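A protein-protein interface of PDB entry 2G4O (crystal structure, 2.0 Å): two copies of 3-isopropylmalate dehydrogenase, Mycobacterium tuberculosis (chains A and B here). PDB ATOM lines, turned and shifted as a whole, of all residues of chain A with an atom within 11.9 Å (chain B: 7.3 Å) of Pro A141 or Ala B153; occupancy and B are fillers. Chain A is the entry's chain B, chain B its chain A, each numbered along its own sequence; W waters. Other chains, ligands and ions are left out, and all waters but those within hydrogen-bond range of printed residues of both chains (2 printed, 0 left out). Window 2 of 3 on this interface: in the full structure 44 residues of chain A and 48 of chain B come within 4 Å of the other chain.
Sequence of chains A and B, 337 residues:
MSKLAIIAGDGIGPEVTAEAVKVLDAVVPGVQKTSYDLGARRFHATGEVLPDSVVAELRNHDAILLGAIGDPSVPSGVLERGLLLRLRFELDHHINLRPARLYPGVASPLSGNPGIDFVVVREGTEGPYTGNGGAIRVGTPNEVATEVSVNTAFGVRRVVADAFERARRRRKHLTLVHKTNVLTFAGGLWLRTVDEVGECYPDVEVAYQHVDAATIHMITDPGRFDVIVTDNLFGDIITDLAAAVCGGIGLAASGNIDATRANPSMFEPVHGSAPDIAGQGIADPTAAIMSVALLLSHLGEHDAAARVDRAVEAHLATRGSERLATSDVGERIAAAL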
ATOM      1  N   GLY A 134      -5.496  17.738 -31.245  1.00  0.00           N
ATOM      2  CA  GLY A 134      -4.733  18.820 -30.647  1.00  0.00           C
ATOM      3  C   GLY A 134      -4.560  18.505 -29.172  1.00  0.00           C
ATOM      4  O   GLY A 134      -5.067  17.484 -28.691  1.00  0.00           O
ATOM      5  N   ALA A 135      -3.932  19.433 -28.458  1.00  0.00           N
ATOM      6  CA  ALA A 135      -3.763  19.356 -27.001  1.00  0.00           C
ATOM      7  C   ALA A 135      -3.769  20.730 -26.355  1.00  0.00           C
ATOM      8  O   ALA A 135      -3.372  21.703 -27.021  1.00  0.00           O
ATOM      9  CB  ALA A 135      -2.482  18.693 -26.670  1.00  0.00           C
ATOM     10  N   ILE A 136      -4.221  20.796 -25.096  1.00  0.00           N
ATOM     11  CA  ILE A 136      -4.097  22.007 -24.292  1.00  0.00           C
ATOM     12  C   ILE A 136      -3.349  21.673 -23.037  1.00  0.00           C
ATOM     13  O   ILE A 136      -3.354  20.522 -22.585  1.00  0.00           O
ATOM     14  CB  ILE A 136      -5.453  22.643 -23.961  1.00  0.00           C
ATOM     15  CG1 ILE A 136      -6.343  21.633 -23.246  1.00  0.00           C
ATOM     16  CG2 ILE A 136      -6.062  23.207 -25.226  1.00  0.00           C
ATOM     17  CD1 ILE A 136      -7.581  22.270 -22.613  1.00  0.00           C
ATOM     18  N   ARG A 137      -2.643  22.689 -22.508  1.00  0.00           N
ATOM     19  CA  ARG A 137      -1.914  22.586 -21.236  1.00  0.00           C
ATOM     20  C   ARG A 137      -0.899  21.469 -21.168  1.00  0.00           C
ATOM     21  O   ARG A 137      -0.789  20.770 -20.155  1.00  0.00           O
ATOM     22  CB  ARG A 137      -2.924  22.527 -20.087  1.00  0.00           C
ATOM     23  CG  ARG A 137      -3.880  23.718 -20.065  1.00  0.00           C
ATOM     24  CD  ARG A 137      -4.854  23.730 -18.853  1.00  0.00           C
ATOM     25  NE  ARG A 137      -5.711  24.905 -19.002  1.00  0.00           N
ATOM     26  CZ  ARG A 137      -7.034  24.923 -19.221  1.00  0.00           C
ATOM     27  NH1 ARG A 137      -7.760  23.829 -19.221  1.00  0.00           N
ATOM     28  NH2 ARG A 137      -7.616  26.049 -19.457  1.00  0.00           N
ATOM     29  N   VAL A 138      -0.135  21.327 -22.249  1.00  0.00           N
ATOM     30  CA  VAL A 138       0.760  20.241 -22.418  1.00  0.00           C
ATOM     31  C   VAL A 138       1.805  20.335 -21.324  1.00  0.00           C
ATOM     32  O   VAL A 138       2.266  21.427 -20.976  1.00  0.00           O
ATOM     33  CB  VAL A 138       1.405  20.169 -23.856  1.00  0.00           C
ATOM     34  CG1 VAL A 138       2.581  19.201 -23.943  1.00  0.00           C
ATOM     35  CG2 VAL A 138       0.424  19.761 -24.876  1.00  0.00           C
ATOM     36  N   GLY A 139       2.120  19.176 -20.745  1.00  0.00           N
ATOM     37  CA  GLY A 139       3.217  19.021 -19.807  1.00  0.00           C
ATOM     38  C   GLY A 139       2.868  19.389 -18.399  1.00  0.00           C
ATOM     39  O   GLY A 139       3.772  19.618 -17.594  1.00  0.00           O
ATOM     40  N   THR A 140       1.582  19.412 -18.105  1.00  0.00           N
ATOM     41  CA  THR A 140       1.029  19.733 -16.786  1.00  0.00           C
ATOM     42  C   THR A 140       0.023  18.626 -16.409  1.00  0.00           C
ATOM     43  O   THR A 140      -0.372  17.853 -17.249  1.00  0.00           O
ATOM     44  CB  THR A 140       0.225  21.050 -16.797  1.00  0.00           C
ATOM     45  OG1 THR A 140      -1.059  20.872 -17.440  1.00  0.00           O
ATOM     46  CG2 THR A 140       1.046  22.174 -17.471  1.00  0.00           C
ATOM     47  N   PRO A 141      -0.336  18.528 -15.154  1.00  0.00           N
ATOM     48  CA  PRO A 141      -1.436  17.661 -14.729  1.00  0.00           C
ATOM     49  C   PRO A 141      -2.807  17.977 -15.364  1.00  0.00           C
ATOM     50  O   PRO A 141      -3.724  17.184 -15.246  1.00  0.00           O
ATOM     51  CB  PRO A 141      -1.514  17.880 -13.197  1.00  0.00           C
ATOM     52  CG  PRO A 141      -0.567  18.985 -12.858  1.00  0.00           C
ATOM     53  CD  PRO A 141       0.340  19.215 -14.024  1.00  0.00           C
ATOM     54  N   ASN A 142      -2.962  19.171 -15.912  1.00  0.00           N
ATOM     55  CA  ASN A 142      -4.184  19.600 -16.638  1.00  0.00           C
ATOM     56  C   ASN A 142      -4.150  19.395 -18.151  1.00  0.00           C
ATOM     57  O   ASN A 142      -5.067  19.878 -18.837  1.00  0.00           O
ATOM     58  CB  ASN A 142      -4.432  21.071 -16.334  1.00  0.00           C
ATOM     59  CG  ASN A 142      -4.066  21.395 -14.898  1.00  0.00           C
ATOM     60  OD1 ASN A 142      -4.714  20.905 -14.010  1.00  0.00           O
ATOM     61  ND2 ASN A 142      -2.949  22.090 -14.691  1.00  0.00           N
ATOM     62  N   GLU A 143      -3.111  18.749 -18.669  1.00  0.00           N
ATOM     63  CA  GLU A 143      -3.071  18.403 -20.115  1.00  0.00           C
ATOM     64  C   GLU A 143      -4.312  17.586 -20.587  1.00  0.00           C
ATOM     65  O   GLU A 143      -4.733  16.627 -19.919  1.00  0.00           O
ATOM     66  CB  GLU A 143      -1.838  17.624 -20.464  1.00  0.00           C
ATOM     67  CG  GLU A 143      -1.700  17.405 -21.979  1.00  0.00           C
ATOM     68  CD  GLU A 143      -0.383  16.802 -22.381  1.00  0.00           C
ATOM     69  OE1 GLU A 143       0.545  16.828 -21.536  1.00  0.00           O
ATOM     70  OE2 GLU A 143      -0.304  16.271 -23.540  1.00  0.00           O
ATOM     71  N   VAL A 144      -4.900  18.017 -21.701  1.00  0.00           N
ATOM     72  CA  VAL A 144      -5.984  17.302 -22.321  1.00  0.00           C
ATOM     73  C   VAL A 144      -5.603  17.177 -23.829  1.00  0.00           C
ATOM     74  O   VAL A 144      -5.273  18.178 -24.492  1.00  0.00           O
ATOM     75  CB  VAL A 144      -7.331  18.026 -22.161  1.00  0.00           C
ATOM     76  CG1 VAL A 144      -8.480  17.287 -22.969  1.00  0.00           C
ATOM     77  CG2 VAL A 144      -7.682  18.295 -20.744  1.00  0.00           C
ATOM     78  N   ALA A 145      -5.699  15.986 -24.378  1.00  0.00           N
ATOM     79  CA  ALA A 145      -5.327  15.732 -25.775  1.00  0.00           C
ATOM     80  C   ALA A 145      -6.502  14.978 -26.460  1.00  0.00           C
ATOM     81  O   ALA A 145      -7.043  13.966 -25.895  1.00  0.00           O
ATOM     82  CB  ALA A 145      -4.110  14.908 -25.834  1.00  0.00           C
ATOM     83  N   THR A 146      -6.828  15.416 -27.686  1.00  0.00           N
ATOM     84  CA  THR A 146      -7.983  14.902 -28.390  1.00  0.00           C
ATOM     85  C   THR A 146      -7.445  14.346 -29.689  1.00  0.00           C
ATOM     86  O   THR A 146      -6.444  14.857 -30.194  1.00  0.00           O
ATOM     87  CB  THR A 146      -9.031  16.012 -28.653  1.00  0.00           C
ATOM     88  OG1 THR A 146      -8.395  17.059 -29.350  1.00  0.00           O
ATOM     89  CG2 THR A 146      -9.557  16.573 -27.384  1.00  0.00           C
ATOM     90  N   GLU B 126     -11.736   6.918 -20.235  1.00  0.00           N
ATOM     91  CA  GLU B 126     -11.599   7.998 -21.173  1.00  0.00           C
ATOM     92  C   GLU B 126     -11.271   7.399 -22.504  1.00  0.00           C
ATOM     93  O   GLU B 126     -11.620   6.230 -22.791  1.00  0.00           O
ATOM     94  CB  GLU B 126     -10.575   9.043 -20.689  1.00  0.00           C
ATOM     95  CG  GLU B 126      -9.104   8.591 -20.445  1.00  0.00           C
ATOM     96  CD  GLU B 126      -8.198   9.732 -20.051  1.00  0.00           C
ATOM     97  OE1 GLU B 126      -8.591  10.484 -19.132  1.00  0.00           O
ATOM     98  OE2 GLU B 126      -7.100   9.817 -20.658  1.00  0.00           O
ATOM     99  N   ASN B 151      -8.372  12.379 -24.042  1.00  0.00           N
ATOM    100  CA  ASN B 151      -7.321  11.849 -23.168  1.00  0.00           C
ATOM    101  C   ASN B 151      -6.803  12.933 -22.258  1.00  0.00           C
ATOM    102  O   ASN B 151      -6.699  14.081 -22.679  1.00  0.00           O
ATOM    103  CB  ASN B 151      -6.201  11.320 -24.007  1.00  0.00           C
ATOM    104  CG  ASN B 151      -6.690  10.341 -25.079  1.00  0.00           C
ATOM    105  OD1 ASN B 151      -6.699   9.139 -24.850  1.00  0.00           O
ATOM    106  ND2 ASN B 151      -7.197  10.866 -26.223  1.00  0.00           N
ATOM    107  N   THR B 152      -6.551  12.589 -21.001  1.00  0.00           N
ATOM    108  CA  THR B 152      -6.101  13.529 -19.982  1.00  0.00           C
ATOM    109  C   THR B 152      -4.912  13.027 -19.174  1.00  0.00           C
ATOM    110  O   THR B 152      -4.829  11.825 -18.820  1.00  0.00           O
ATOM    111  CB  THR B 152      -7.262  13.813 -19.019  1.00  0.00           C
ATOM    112  OG1 THR B 152      -7.540  12.654 -18.203  1.00  0.00           O
ATOM    113  CG2 THR B 152      -8.519  14.206 -19.812  1.00  0.00           C
ATOM    114  N   ALA B 153      -4.005  13.946 -18.854  1.00  0.00           N
ATOM    115  CA  ALA B 153      -2.968  13.704 -17.884  1.00  0.00           C
ATOM    116  C   ALA B 153      -3.480  13.117 -16.587  1.00  0.00           C
ATOM    117  O   ALA B 153      -2.868  12.168 -16.080  1.00  0.00           O
ATOM    118  CB  ALA B 153      -2.158  14.873 -17.645  1.00  0.00           C
ATOM    119  N   PHE B 154      -4.599  13.606 -16.095  1.00  0.00           N
ATOM    120  CA  PHE B 154      -5.326  13.051 -14.927  1.00  0.00           C
ATOM    121  C   PHE B 154      -5.547  11.526 -15.064  1.00  0.00           C
ATOM    122  O   PHE B 154      -5.123  10.736 -14.218  1.00  0.00           O
ATOM    123  CB  PHE B 154      -6.707  13.707 -14.732  1.00  0.00           C
ATOM    124  CG  PHE B 154      -7.487  13.173 -13.571  1.00  0.00           C
ATOM    125  CD1 PHE B 154      -7.082  13.417 -12.276  1.00  0.00           C
ATOM    126  CD2 PHE B 154      -8.658  12.477 -13.747  1.00  0.00           C
ATOM    127  CE1 PHE B 154      -7.804  12.933 -11.198  1.00  0.00           C
ATOM    128  CE2 PHE B 154      -9.376  12.007 -12.649  1.00  0.00           C
ATOM    129  CZ  PHE B 154      -8.956  12.226 -11.405  1.00  0.00           C
ATOM    130  N   GLY B 155      -6.183  11.167 -16.155  1.00  0.00           N
ATOM    131  CA  GLY B 155      -6.537   9.797 -16.438  1.00  0.00           C
ATOM    132  C   GLY B 155      -5.346   8.946 -16.718  1.00  0.00           C
ATOM    133  O   GLY B 155      -5.207   7.844 -16.133  1.00  0.00           O
ATOM    134  N   VAL B 156      -4.507   9.411 -17.630  1.00  0.00           N
ATOM    135  CA  VAL B 156      -3.316   8.655 -17.961  1.00  0.00           C
ATOM    136  C   VAL B 156      -2.344   8.407 -16.818  1.00  0.00           C
ATOM    137  O   VAL B 156      -1.918   7.274 -16.622  1.00  0.00           O
ATOM    138  CB  VAL B 156      -2.639   9.241 -19.160  1.00  0.00           C
ATOM    139  CG1 VAL B 156      -1.412   8.452 -19.479  1.00  0.00           C
ATOM    140  CG2 VAL B 156      -3.621   9.176 -20.338  1.00  0.00           C
ATOM    141  N   ARG B 157      -1.997   9.444 -16.056  1.00  0.00           N
ATOM    142  CA  ARG B 157      -1.054   9.299 -15.000  1.00  0.00           C
ATOM    143  C   ARG B 157      -1.483   8.211 -14.026  1.00  0.00           C
ATOM    144  O   ARG B 157      -0.637   7.489 -13.523  1.00  0.00           O
ATOM    145  CB  ARG B 157      -0.821  10.599 -14.228  1.00  0.00           C
ATOM    146  CG  ARG B 157       0.548  10.575 -13.572  1.00  0.00           C
ATOM    147  CD  ARG B 157       0.814  11.635 -12.491  1.00  0.00           C
ATOM    148  NE  ARG B 157       2.140  11.507 -11.825  1.00  0.00           N
ATOM    149  CZ  ARG B 157       2.415  10.651 -10.842  1.00  0.00           C
ATOM    150  NH1 ARG B 157       1.488   9.832 -10.373  1.00  0.00           N
ATOM    151  NH2 ARG B 157       3.630  10.620 -10.311  1.00  0.00           N
ATOM    152  N   ARG B 158      -2.788   8.141 -13.751  1.00  0.00           N
ATOM    153  CA  ARG B 158      -3.410   7.195 -12.789  1.00  0.00           C
ATOM    154  C   ARG B 158      -3.053   5.771 -13.098  1.00  0.00           C
ATOM    155  O   ARG B 158      -2.518   5.011 -12.287  1.00  0.00           O
ATOM    156  CB  ARG B 158      -4.954   7.243 -12.920  1.00  0.00           C
ATOM    157  CG  ARG B 158      -5.506   8.534 -12.598  1.00  0.00           C
ATOM    158  CD  ARG B 158      -6.832   8.524 -11.976  1.00  0.00           C
ATOM    159  NE  ARG B 158      -7.819   8.378 -13.000  1.00  0.00           N
ATOM    160  CZ  ARG B 158      -9.100   8.519 -12.770  1.00  0.00           C
ATOM    161  NH1 ARG B 158      -9.520   8.792 -11.530  1.00  0.00           N
ATOM    162  NH2 ARG B 158      -9.933   8.368 -13.758  1.00  0.00           N
ATOM    163  N   VAL B 159      -3.372   5.449 -14.344  1.00  0.00           N
ATOM    164  CA  VAL B 159      -3.276   4.118 -14.885  1.00  0.00           C
ATOM    165  C   VAL B 159      -1.800   3.746 -15.055  1.00  0.00           C
ATOM    166  O   VAL B 159      -1.417   2.611 -14.770  1.00  0.00           O
ATOM    167  CB  VAL B 159      -4.042   4.041 -16.207  1.00  0.00           C
ATOM    168  CG1 VAL B 159      -3.856   2.699 -16.908  1.00  0.00           C
ATOM    169  CG2 VAL B 159      -5.510   4.340 -15.945  1.00  0.00           C
ATOM    170  N   LEU B 189       0.975  12.241 -25.081  1.00  0.00           N
ATOM    171  CA  LEU B 189       0.592  12.327 -23.689  1.00  0.00           C
ATOM    172  C   LEU B 189       1.035  11.058 -22.979  1.00  0.00           C
ATOM    173  O   LEU B 189       1.656  11.135 -21.911  1.00  0.00           O
ATOM    174  CB  LEU B 189      -0.897  12.550 -23.491  1.00  0.00           C
ATOM    175  CG  LEU B 189      -1.396  12.428 -22.072  1.00  0.00           C
ATOM    176  CD1 LEU B 189      -0.789  13.421 -21.132  1.00  0.00           C
ATOM    177  CD2 LEU B 189      -2.954  12.503 -22.140  1.00  0.00           C
ATOM    178  N   ARG B 192       5.050  10.615 -22.724  1.00  0.00           N
ATOM    179  CA  ARG B 192       5.634  11.509 -21.719  1.00  0.00           C
ATOM    180  C   ARG B 192       5.220  11.125 -20.353  1.00  0.00           C
ATOM    181  O   ARG B 192       6.013  11.267 -19.392  1.00  0.00           O
ATOM    182  CB  ARG B 192       5.239  12.985 -21.975  1.00  0.00           C
ATOM    183  CG  ARG B 192       5.993  13.553 -23.176  1.00  0.00           C
ATOM    184  CD  ARG B 192       5.627  14.988 -23.584  1.00  0.00           C
ATOM    185  NE  ARG B 192       4.383  15.125 -24.376  1.00  0.00           N
ATOM    186  CZ  ARG B 192       3.219  15.467 -23.866  1.00  0.00           C
ATOM    187  NH1 ARG B 192       3.091  15.689 -22.550  1.00  0.00           N
ATOM    188  NH2 ARG B 192       2.184  15.614 -24.671  1.00  0.00           N
ATOM    189  N   THR B 193       4.002  10.584 -20.237  1.00  0.00           N
ATOM    190  CA  THR B 193       3.545  10.216 -18.929  1.00  0.00           C
ATOM    191  C   THR B 193       4.304   9.010 -18.399  1.00  0.00           C
ATOM    192  O   THR B 193       4.757   8.985 -17.217  1.00  0.00           O
ATOM    193  CB  THR B 193       2.007  10.045 -18.896  1.00  0.00           C
ATOM    194  OG1 THR B 193       1.400  11.277 -19.284  1.00  0.00           O
ATOM    195  CG2 THR B 193       1.598   9.719 -17.521  1.00  0.00           C
HETATM  196  O   HOH W   1      -0.475  15.932 -26.239  1.00  0.00           O
HETATM  197  O   HOH W   2      -5.520  16.361 -17.215  1.00  0.00           O
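Val A138 touches Arg B192 (CG1 to NH2, 3.7 Å).
Ala B153 touches Thr A140.
O of Pro A141 touches CB of Ala B153, 3.7 Å away.
N of Phe B154 touches O of Pro A141 (3.8 Å).
O of Glu A143 touches CA of Thr B152, at 3.4 Å.
CD of Glu A143 touches CD1 of Leu B189, at 3.6 Å.
Val A144 touches Asn B151.
O of Glu A143 is in hydrogen-bond range of N of Ala B153 (3.0 Å).
The backbone NH of Ala A145 sits at hydrogen-bond distance from the backbone carbonyl oxygen of Asn B151, 2.7 Å away.
The guanidinium group (NH2) of Arg B192 lies within salt-bridge range of the side-chain carboxylate (OE2) of Glu A143 (2.8 Å).
Water W1 bridges OE2 of Glu A143 (2.7 Å) and NH2 of Arg B192 (3.1 Å).
Water W2 lies within hydrogen-bond range of the backbone carbonyl oxygen (O) of Pro A141, the backbone carbonyl oxygen (O) of Glu A143, the backbone NH (N) of Phe B154 and the backbone NH (N) of Ala B153.
Of the 13 printed residues of chain A, 6 touch a printed residue of chain B.
Hydrophobic or aromatic side chains of chain A within 4 Å of the printed part of chain B: Val A138 and Val A144.
Of the 13 printed residues of chain B, 6 touch a printed residue of chain A.
Hydrophobic or aromatic side chains of chain B within 4 Å of the printed part of chain A: Ala B153 and Leu B189.
Among the printed residues, 10 pairs touch across the chains.
Among the printed residues, Asp or Glu carboxylates within 4 Å of a Lys or Arg side-chain nitrogen of the other chain: Glu A143 with Arg B192 (2.8 Å).
No position is printed for both chains.
Of the 10 pairs that touch across the chains among the printed residues, none has its exchanged pair printed and touching as well.
OG1 of Thr A140 lies within hydrogen-bond range of N of Asn A142 (3.0 Å).
N of Gly A139 is in hydrogen-bond range of OE1 of Glu A143 (2.9 Å).
The side-chain hydroxyl of Thr B152 sits at hydrogen-bond distance from the backbone NH of Gly B155 (2.9 Å).
The backbone carbonyl oxygen (O) of Arg A137 sits close to the backbone NH (N) of Glu A143, 3.4 Å away.
The side-chain hydroxyl (OG1) of Thr A140 lies within hydrogen-bond range of the backbone NH (N) of Glu A143 (3.2 Å).
OE1 of Glu B126 sits at hydrogen-bond distance from OG1 of Thr B152, at 2.6 Å.
Ile A136 touches none of the printed residues of chain B.
Arg A137 touches none of the printed residues of chain B.
Printed residues of chain B within 4 Å of Glu A143: Thr B152, Ala B153, Leu B189 and Arg B192.
Thr B152 touches just one residue of chain A: Glu A143 (3.4 Å).
Ala B153 touches three residues of chain A.
Of chain A, only Pro A141 (3.8 Å) comes within 4 Å of Phe B154.
No residue of chain A comes within 4 Å of Gly B155.
No residue of chain A comes within 4 Å of Val B156.
Of the printed residues of chain A, Leu B189 touches Glu A143.
Of the printed residues of chain A, Arg B192 touches Val A138 (3.7 Å) and Glu A143 (2.8 Å).
The nearest residue of chain B that does not touch Pro A141 is Thr B152 (5.8 Å).
The nearest residue of chain A that does not touch Ala B153 is Asn A142 (4.7 Å).
The nearest printed residue of chain A that does not touch Leu B189 is Ala A145 (4.6 Å).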
